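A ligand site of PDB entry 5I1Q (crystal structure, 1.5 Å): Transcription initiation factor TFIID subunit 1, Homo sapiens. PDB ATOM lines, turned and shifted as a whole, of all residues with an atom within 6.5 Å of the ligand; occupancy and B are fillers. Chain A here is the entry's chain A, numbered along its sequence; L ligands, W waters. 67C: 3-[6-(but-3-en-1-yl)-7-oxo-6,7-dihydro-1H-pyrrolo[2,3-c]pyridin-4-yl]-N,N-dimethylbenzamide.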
ATOM      1  N   TRP A  32       7.505  -1.500 -10.175  1.00  0.00           N
ATOM      2  CA  TRP A  32       6.054  -1.026 -10.385  1.00  0.00           C
ATOM      3  C   TRP A  32       5.932   0.389 -10.996  1.00  0.00           C
ATOM      4  O   TRP A  32       4.956   0.546 -11.734  1.00  0.00           O
ATOM      5  CB  TRP A  32       5.273  -1.164  -9.068  1.00  0.00           C
ATOM      6  CG  TRP A  32       5.817  -0.262  -7.995  1.00  0.00           C
ATOM      7  CD1 TRP A  32       6.750  -0.630  -7.048  1.00  0.00           C
ATOM      8  CD2 TRP A  32       5.600   1.137  -7.822  1.00  0.00           C
ATOM      9  NE1 TRP A  32       7.122   0.460  -6.273  1.00  0.00           N
ATOM     10  CE2 TRP A  32       6.411   1.572  -6.738  1.00  0.00           C
ATOM     11  CE3 TRP A  32       4.763   2.105  -8.464  1.00  0.00           C
ATOM     12  CZ2 TRP A  32       6.432   2.912  -6.316  1.00  0.00           C
ATOM     13  CZ3 TRP A  32       4.782   3.438  -8.019  1.00  0.00           C
ATOM     14  CH2 TRP A  32       5.615   3.820  -6.947  1.00  0.00           C
ATOM     15  N   PRO A  33       6.857   1.350 -10.739  1.00  0.00           N
ATOM     16  CA  PRO A  33       6.530   2.682 -11.339  1.00  0.00           C
ATOM     17  C   PRO A  33       6.492   2.616 -12.851  1.00  0.00           C
ATOM     18  O   PRO A  33       5.833   3.508 -13.470  1.00  0.00           O
ATOM     19  CB  PRO A  33       7.765   3.559 -10.943  1.00  0.00           C
ATOM     20  CG  PRO A  33       8.233   2.895  -9.614  1.00  0.00           C
ATOM     21  CD  PRO A  33       8.042   1.414  -9.834  1.00  0.00           C
ATOM     22  N   PHE A  34       7.133   1.605 -13.467  1.00  0.00           N
ATOM     23  CA  PHE A  34       7.295   1.552 -14.948  1.00  0.00           C
ATOM     24  C   PHE A  34       6.310   0.550 -15.565  1.00  0.00           C
ATOM     25  O   PHE A  34       6.370   0.378 -16.789  1.00  0.00           O
ATOM     26  CB  PHE A  34       8.772   1.127 -15.252  1.00  0.00           C
ATOM     27  CG  PHE A  34       9.731   2.082 -14.633  1.00  0.00           C
ATOM     28  CD1 PHE A  34       9.915   3.338 -15.217  1.00  0.00           C
ATOM     29  CD2 PHE A  34      10.410   1.804 -13.412  1.00  0.00           C
ATOM     30  CE1 PHE A  34      10.729   4.300 -14.657  1.00  0.00           C
ATOM     31  CE2 PHE A  34      11.260   2.748 -12.798  1.00  0.00           C
ATOM     32  CZ  PHE A  34      11.443   4.001 -13.426  1.00  0.00           C
ATOM     33  N   HIS A  35       5.462  -0.125 -14.795  1.00  0.00           N
ATOM     34  CA  HIS A  35       4.587  -1.190 -15.320  1.00  0.00           C
ATOM     35  C   HIS A  35       3.490  -0.701 -16.234  1.00  0.00           C
ATOM     36  O   HIS A  35       3.094  -1.450 -17.123  1.00  0.00           O
ATOM     37  CB  HIS A  35       4.047  -2.008 -14.144  1.00  0.00           C
ATOM     38  CG  HIS A  35       5.087  -2.890 -13.498  1.00  0.00           C
ATOM     39  ND1 HIS A  35       4.702  -3.692 -12.468  1.00  0.00           N
ATOM     40  CD2 HIS A  35       6.453  -2.918 -13.557  1.00  0.00           C
ATOM     41  CE1 HIS A  35       5.797  -4.345 -12.042  1.00  0.00           C
ATOM     42  NE2 HIS A  35       6.844  -3.935 -12.695  1.00  0.00           N
ATOM     43  N   HIS A  36       3.004   0.515 -15.935  1.00  0.00           N
ATOM     44  CA  HIS A  36       1.773   1.007 -16.595  1.00  0.00           C
ATOM     45  C   HIS A  36       1.985   2.474 -16.901  1.00  0.00           C
ATOM     46  O   HIS A  36       2.831   3.138 -16.275  1.00  0.00           O
ATOM     47  CB  HIS A  36       0.550   0.854 -15.637  1.00  0.00           C
ATOM     48  CG  HIS A  36       0.277  -0.565 -15.286  1.00  0.00           C
ATOM     49  ND1 HIS A  36      -0.283  -1.462 -16.177  1.00  0.00           N
ATOM     50  CD2 HIS A  36       0.582  -1.259 -14.140  1.00  0.00           C
ATOM     51  CE1 HIS A  36      -0.319  -2.676 -15.585  1.00  0.00           C
ATOM     52  NE2 HIS A  36       0.159  -2.557 -14.339  1.00  0.00           N
ATOM     53  N   PRO A  37       1.183   3.054 -17.852  1.00  0.00           N
ATOM     54  CA  PRO A  37       1.278   4.488 -18.039  1.00  0.00           C
ATOM     55  C   PRO A  37       0.966   5.266 -16.736  1.00  0.00           C
ATOM     56  O   PRO A  37       0.127   4.882 -15.928  1.00  0.00           O
ATOM     57  CB  PRO A  37       0.183   4.786 -19.099  1.00  0.00           C
ATOM     58  CG  PRO A  37      -0.444   3.529 -19.426  1.00  0.00           C
ATOM     59  CD  PRO A  37       0.113   2.386 -18.610  1.00  0.00           C
ATOM     60  N   VAL A  38       1.639   6.427 -16.650  1.00  0.00           N
ATOM     61  CA  VAL A  38       1.423   7.308 -15.489  1.00  0.00           C
ATOM     62  C   VAL A  38       0.032   7.909 -15.534  1.00  0.00           C
ATOM     63  O   VAL A  38      -0.390   8.356 -16.618  1.00  0.00           O
ATOM     64  CB  VAL A  38       2.441   8.472 -15.564  1.00  0.00           C
ATOM     65  CG1 VAL A  38       2.151   9.403 -14.397  1.00  0.00           C
ATOM     66  CG2 VAL A  38       3.849   7.851 -15.400  1.00  0.00           C
ATOM     67  N   ASN A  39      -0.646   7.950 -14.423  1.00  0.00           N
ATOM     68  CA  ASN A  39      -2.001   8.622 -14.327  1.00  0.00           C
ATOM     69  C   ASN A  39      -1.709   9.948 -13.709  1.00  0.00           C
ATOM     70  O   ASN A  39      -1.166  10.037 -12.610  1.00  0.00           O
ATOM     71  CB  ASN A  39      -2.856   7.769 -13.376  1.00  0.00           C
ATOM     72  CG  ASN A  39      -4.307   8.194 -13.298  1.00  0.00           C
ATOM     73  OD1 ASN A  39      -4.627   9.374 -13.404  1.00  0.00           O
ATOM     74  ND2 ASN A  39      -5.189   7.194 -13.087  1.00  0.00           N
ATOM     75  N   LYS A  40      -2.161  11.002 -14.420  1.00  0.00           N
ATOM     76  CA  LYS A  40      -1.971  12.356 -13.898  1.00  0.00           C
ATOM     77  C   LYS A  40      -2.715  12.635 -12.625  1.00  0.00           C
ATOM     78  O   LYS A  40      -2.238  13.521 -11.867  1.00  0.00           O
ATOM     79  CB  LYS A  40      -2.407  13.396 -14.987  1.00  0.00           C
ATOM     80  CG  LYS A  40      -3.896  13.282 -15.349  1.00  0.00           C
ATOM     81  CD  LYS A  40      -4.580  14.561 -14.887  1.00  0.00           C
ATOM     82  CE  LYS A  40      -6.065  14.672 -15.267  1.00  0.00           C
ATOM     83  NZ  LYS A  40      -6.405  16.120 -15.576  1.00  0.00           N
ATOM     84  N   PHE A  42      -2.253  10.744 -10.141  1.00  0.00           N
ATOM     85  CA  PHE A  42      -1.222  10.221  -9.145  1.00  0.00           C
ATOM     86  C   PHE A  42       0.061  11.019  -9.260  1.00  0.00           C
ATOM     87  O   PHE A  42       0.833  11.082  -8.255  1.00  0.00           O
ATOM     88  CB  PHE A  42      -1.013   8.711  -9.377  1.00  0.00           C
ATOM     89  CG  PHE A  42      -2.253   7.877  -9.305  1.00  0.00           C
ATOM     90  CD1 PHE A  42      -3.476   8.331  -8.694  1.00  0.00           C
ATOM     91  CD2 PHE A  42      -2.230   6.687  -9.954  1.00  0.00           C
ATOM     92  CE1 PHE A  42      -4.614   7.487  -8.687  1.00  0.00           C
ATOM     93  CE2 PHE A  42      -3.386   5.841  -9.949  1.00  0.00           C
ATOM     94  CZ  PHE A  42      -4.540   6.257  -9.303  1.00  0.00           C
ATOM     95  N   VAL A  43       0.386  11.548 -10.452  1.00  0.00           N
ATOM     96  CA  VAL A  43       1.638  12.324 -10.698  1.00  0.00           C
ATOM     97  C   VAL A  43       1.286  13.572 -11.531  1.00  0.00           C
ATOM     98  O   VAL A  43       1.344  13.542 -12.736  1.00  0.00           O
ATOM     99  CB  VAL A  43       2.713  11.464 -11.387  1.00  0.00           C
ATOM    100  CG1 VAL A  43       4.038  12.268 -11.365  1.00  0.00           C
ATOM    101  CG2 VAL A  43       2.953  10.070 -10.692  1.00  0.00           C
ATOM    102  N   TYR A  46       3.540  15.070 -14.375  1.00  0.00           N
ATOM    103  CA  TYR A  46       4.261  14.223 -15.292  1.00  0.00           C
ATOM    104  C   TYR A  46       4.363  14.608 -16.733  1.00  0.00           C
ATOM    105  O   TYR A  46       5.434  14.693 -17.337  1.00  0.00           O
ATOM    106  CB  TYR A  46       3.842  12.723 -15.086  1.00  0.00           C
ATOM    107  CG  TYR A  46       4.785  11.744 -15.767  1.00  0.00           C
ATOM    108  CD1 TYR A  46       5.985  11.468 -15.076  1.00  0.00           C
ATOM    109  CD2 TYR A  46       4.552  11.189 -16.983  1.00  0.00           C
ATOM    110  CE1 TYR A  46       6.871  10.552 -15.648  1.00  0.00           C
ATOM    111  CE2 TYR A  46       5.420  10.268 -17.601  1.00  0.00           C
ATOM    112  CZ  TYR A  46       6.582   9.997 -16.887  1.00  0.00           C
ATOM    113  OH  TYR A  46       7.515   9.136 -17.454  1.00  0.00           O
ATOM    114  N   MET A  54       6.470   6.583 -22.036  1.00  0.00           N
ATOM    115  CA  MET A  54       6.583   5.131 -22.334  1.00  0.00           C
ATOM    116  C   MET A  54       6.503   4.331 -21.071  1.00  0.00           C
ATOM    117  O   MET A  54       6.850   4.787 -19.967  1.00  0.00           O
ATOM    118  CB  MET A  54       7.857   4.832 -23.137  1.00  0.00           C
ATOM    119  CG  MET A  54       8.028   3.403 -23.707  1.00  0.00           C
ATOM    120  SD  MET A  54       6.596   2.787 -24.648  1.00  0.00           S
ATOM    121  CE  MET A  54       6.399   4.091 -25.904  1.00  0.00           C
ATOM    122  N   ASP A  55       5.994   3.092 -21.216  1.00  0.00           N
ATOM    123  CA  ASP A  55       5.923   2.237 -20.047  1.00  0.00           C
ATOM    124  C   ASP A  55       5.902   0.742 -20.522  1.00  0.00           C
ATOM    125  O   ASP A  55       5.750   0.499 -21.726  1.00  0.00           O
ATOM    126  CB  ASP A  55       4.675   2.519 -19.199  1.00  0.00           C
ATOM    127  CG  ASP A  55       3.449   2.219 -20.000  1.00  0.00           C
ATOM    128  OD1 ASP A  55       3.010   3.085 -20.804  1.00  0.00           O
ATOM    129  OD2 ASP A  55       2.970   1.080 -19.917  1.00  0.00           O
ATOM    130  N   LEU A  56       6.053  -0.219 -19.634  1.00  0.00           N
ATOM    131  CA  LEU A  56       6.113  -1.592 -20.035  1.00  0.00           C
ATOM    132  C   LEU A  56       4.797  -2.143 -20.600  1.00  0.00           C
ATOM    133  O   LEU A  56       4.868  -3.027 -21.462  1.00  0.00           O
ATOM    134  CB  LEU A  56       6.682  -2.473 -18.884  1.00  0.00           C
ATOM    135  CG  LEU A  56       8.090  -2.062 -18.423  1.00  0.00           C
ATOM    136  CD1 LEU A  56       8.475  -2.900 -17.227  1.00  0.00           C
ATOM    137  CD2 LEU A  56       9.103  -2.285 -19.490  1.00  0.00           C
ATOM    138  N   ILE A  81      12.196   4.710 -21.768  1.00  0.00           N
ATOM    139  CA  ILE A  81      11.839   4.648 -20.348  1.00  0.00           C
ATOM    140  C   ILE A  81      13.016   5.224 -19.498  1.00  0.00           C
ATOM    141  O   ILE A  81      12.840   6.050 -18.597  1.00  0.00           O
ATOM    142  CB  ILE A  81      11.482   3.203 -19.957  1.00  0.00           C
ATOM    143  CG1 ILE A  81      10.172   2.834 -20.690  1.00  0.00           C
ATOM    144  CG2 ILE A  81      11.292   3.132 -18.460  1.00  0.00           C
ATOM    145  CD1 ILE A  81       9.751   1.384 -20.454  1.00  0.00           C
ATOM    146  N   ASN A  84      13.441   9.013 -20.067  1.00  0.00           N
ATOM    147  CA  ASN A  84      12.396   9.762 -19.418  1.00  0.00           C
ATOM    148  C   ASN A  84      12.566   9.865 -17.914  1.00  0.00           C
ATOM    149  O   ASN A  84      12.305  10.924 -17.244  1.00  0.00           O
ATOM    150  CB  ASN A  84      10.986   9.203 -19.668  1.00  0.00           C
ATOM    151  CG  ASN A  84      10.448   9.502 -21.060  1.00  0.00           C
ATOM    152  OD1 ASN A  84      10.919  10.467 -21.680  1.00  0.00           O
ATOM    153  ND2 ASN A  84       9.557   8.658 -21.538  1.00  0.00           N
ATOM    154  N   SER A  85      13.084   8.761 -17.299  1.00  0.00           N
ATOM    155  CA  SER A  85      13.372   8.813 -15.831  1.00  0.00           C
ATOM    156  C   SER A  85      14.526   9.773 -15.535  1.00  0.00           C
ATOM    157  O   SER A  85      14.453  10.558 -14.542  1.00  0.00           O
ATOM    158  CB  SER A  85      13.729   7.430 -15.249  1.00  0.00           C
ATOM    159  OG  SER A  85      13.753   7.546 -13.857  1.00  0.00           O
ATOM    160  N   TYR A  88      12.837  13.209 -15.737  1.00  0.00           N
ATOM    161  CA  TYR A  88      11.801  13.578 -14.766  1.00  0.00           C
ATOM    162  C   TYR A  88      12.330  13.549 -13.317  1.00  0.00           C
ATOM    163  O   TYR A  88      11.968  14.378 -12.471  1.00  0.00           O
ATOM    164  CB  TYR A  88      10.568  12.629 -14.935  1.00  0.00           C
ATOM    165  CG  TYR A  88       9.402  13.160 -14.108  1.00  0.00           C
ATOM    166  CD1 TYR A  88       8.762  14.321 -14.562  1.00  0.00           C
ATOM    167  CD2 TYR A  88       8.986  12.589 -12.902  1.00  0.00           C
ATOM    168  CE1 TYR A  88       7.728  14.848 -13.813  1.00  0.00           C
ATOM    169  CE2 TYR A  88       7.938  13.182 -12.128  1.00  0.00           C
ATOM    170  CZ  TYR A  88       7.332  14.304 -12.649  1.00  0.00           C
ATOM    171  OH  TYR A  88       6.278  14.873 -11.958  1.00  0.00           O
ATOM    172  N   ASN A  89      13.098  12.495 -13.030  1.00  0.00           N
ATOM    173  CA  ASN A  89      13.582  12.252 -11.653  1.00  0.00           C
ATOM    174  C   ASN A  89      15.045  12.640 -11.400  1.00  0.00           C
ATOM    175  O   ASN A  89      15.410  12.816 -10.223  1.00  0.00           O
ATOM    176  CB  ASN A  89      13.423  10.737 -11.371  1.00  0.00           C
ATOM    177  CG  ASN A  89      11.966  10.299 -11.594  1.00  0.00           C
ATOM    178  OD1 ASN A  89      11.064  10.875 -10.959  1.00  0.00           O
ATOM    179  ND2 ASN A  89      11.760   9.332 -12.470  1.00  0.00           N
ATOM    180  N   TYR A  95      14.400   6.027  -8.764  1.00  0.00           N
ATOM    181  CA  TYR A  95      13.564   5.651  -9.919  1.00  0.00           C
ATOM    182  C   TYR A  95      14.487   5.404 -11.103  1.00  0.00           C
ATOM    183  O   TYR A  95      14.215   4.429 -11.860  1.00  0.00           O
ATOM    184  CB  TYR A  95      12.586   6.786 -10.353  1.00  0.00           C
ATOM    185  CG  TYR A  95      11.421   6.955  -9.455  1.00  0.00           C
ATOM    186  CD1 TYR A  95      10.370   6.017  -9.388  1.00  0.00           C
ATOM    187  CD2 TYR A  95      11.251   8.162  -8.697  1.00  0.00           C
ATOM    188  CE1 TYR A  95       9.271   6.220  -8.572  1.00  0.00           C
ATOM    189  CE2 TYR A  95      10.150   8.341  -7.904  1.00  0.00           C
ATOM    190  CZ  TYR A  95       9.171   7.391  -7.845  1.00  0.00           C
ATOM    191  OH  TYR A  95       8.046   7.547  -7.027  1.00  0.00           O
HETATM  192  C1  67C L   1      -0.403   4.316 -12.466  1.00  0.00           C
HETATM  193  N1  67C L   1       7.442   6.948 -12.708  1.00  0.00           N
HETATM  194  O1  67C L   1       9.241   8.361 -13.051  1.00  0.00           O
HETATM  195  C2  67C L   1       1.051   5.874 -11.364  1.00  0.00           C
HETATM  196  N2  67C L   1       8.485   9.897 -10.598  1.00  0.00           N
HETATM  197  C3  67C L   1       2.232   6.242 -10.470  1.00  0.00           C
HETATM  198  C4  67C L   1       3.464   6.573 -11.055  1.00  0.00           C
HETATM  199  C5  67C L   1       4.563   6.979 -10.234  1.00  0.00           C
HETATM  200  C6  67C L   1       4.330   7.076  -8.872  1.00  0.00           C
HETATM  201  C7  67C L   1       3.086   6.803  -8.320  1.00  0.00           C
HETATM  202  C8  67C L   1       2.014   6.344  -9.092  1.00  0.00           C
HETATM  203  C9  67C L   1       5.807   7.364 -10.914  1.00  0.00           C
HETATM  204  C10 67C L   1       6.317   6.628 -12.039  1.00  0.00           C
HETATM  205  C15 67C L   1       8.323   8.033 -12.351  1.00  0.00           C
HETATM  206  C11 67C L   1       7.838   6.067 -13.860  1.00  0.00           C
HETATM  207  C12 67C L   1       6.847   6.463 -15.030  1.00  0.00           C
HETATM  208  C13 67C L   1       7.186   5.606 -16.211  1.00  0.00           C
HETATM  209  C14 67C L   1       6.356   4.713 -16.733  1.00  0.00           C
HETATM  210  C16 67C L   1       7.847   8.756 -11.159  1.00  0.00           C
HETATM  211  C19 67C L   1       7.666  10.176  -9.588  1.00  0.00           C
HETATM  212  C18 67C L   1       6.505   9.432  -9.345  1.00  0.00           C
HETATM  213  C17 67C L   1       6.684   8.479 -10.439  1.00  0.00           C
HETATM  214  O   67C L   1       0.656   6.826 -12.142  1.00  0.00           O
HETATM  215  N   67C L   1       0.626   4.683 -11.460  1.00  0.00           N
HETATM  216  C   67C L   1       1.222   3.538 -10.734  1.00  0.00           C
HETATM  217  O   HOH W   1       3.193   4.410 -13.797  1.00  0.00           O
HETATM  218  O   HOH W   2      10.363   6.372 -17.327  1.00  0.00           O
HETATM  219  O   HOH W   3       9.871   8.599 -15.801  1.00  0.00           O
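Residues that only touch the ligand: Trp 32 (3.8 Å), Pro 33 (3.3 Å), Phe 34 (3.5 Å), His 36 (3.9 Å), Pro 37 (3.5 Å), Val 38 (3.3 Å), Phe 42 (3.6 Å), Val 43 (3.5 Å), Tyr 46 (3.7 Å), Met 54 (3.3 Å), Asp 55 (3.7 Å), Tyr 88 (3.6 Å) and Tyr 95 (3.4 Å).
Hydrophobic or aromatic side chains within 4 Å of the ligand: Trp 32, Pro 33, Phe 34, Val 38, Phe 42, Val 43, Tyr 88 and Tyr 95.
Of the 21 residues printed, 15 come within 4 Å of the ligand.
Along chain A the residues within 4 Å of the ligand span positions 32 to 95.
The nearest printed residue that does not touch the ligand is Ser 85 (4.7 Å).
The backbone carbonyl oxygen (O) of Phe 34 lies within hydrogen-bond range of the backbone NH (N) of Leu 56.
The side-chain amide nitrogen of Asn 89 is in hydrogen-bond range of the side-chain hydroxyl of Ser 85 (3.0 Å).
The side-chain amide nitrogen (ND2) of Asn 89 sits at hydrogen-bond distance from an oxygen (O1) of the ligand (2.8 Å).
O of the ligand lies within hydrogen-bond range of N of Asn 39 (2.9 Å).
Water W3 bridges an oxygen (O1) of the ligand (2.8 Å) and the side-chain hydroxyl of Tyr 46 (2.9 Å).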
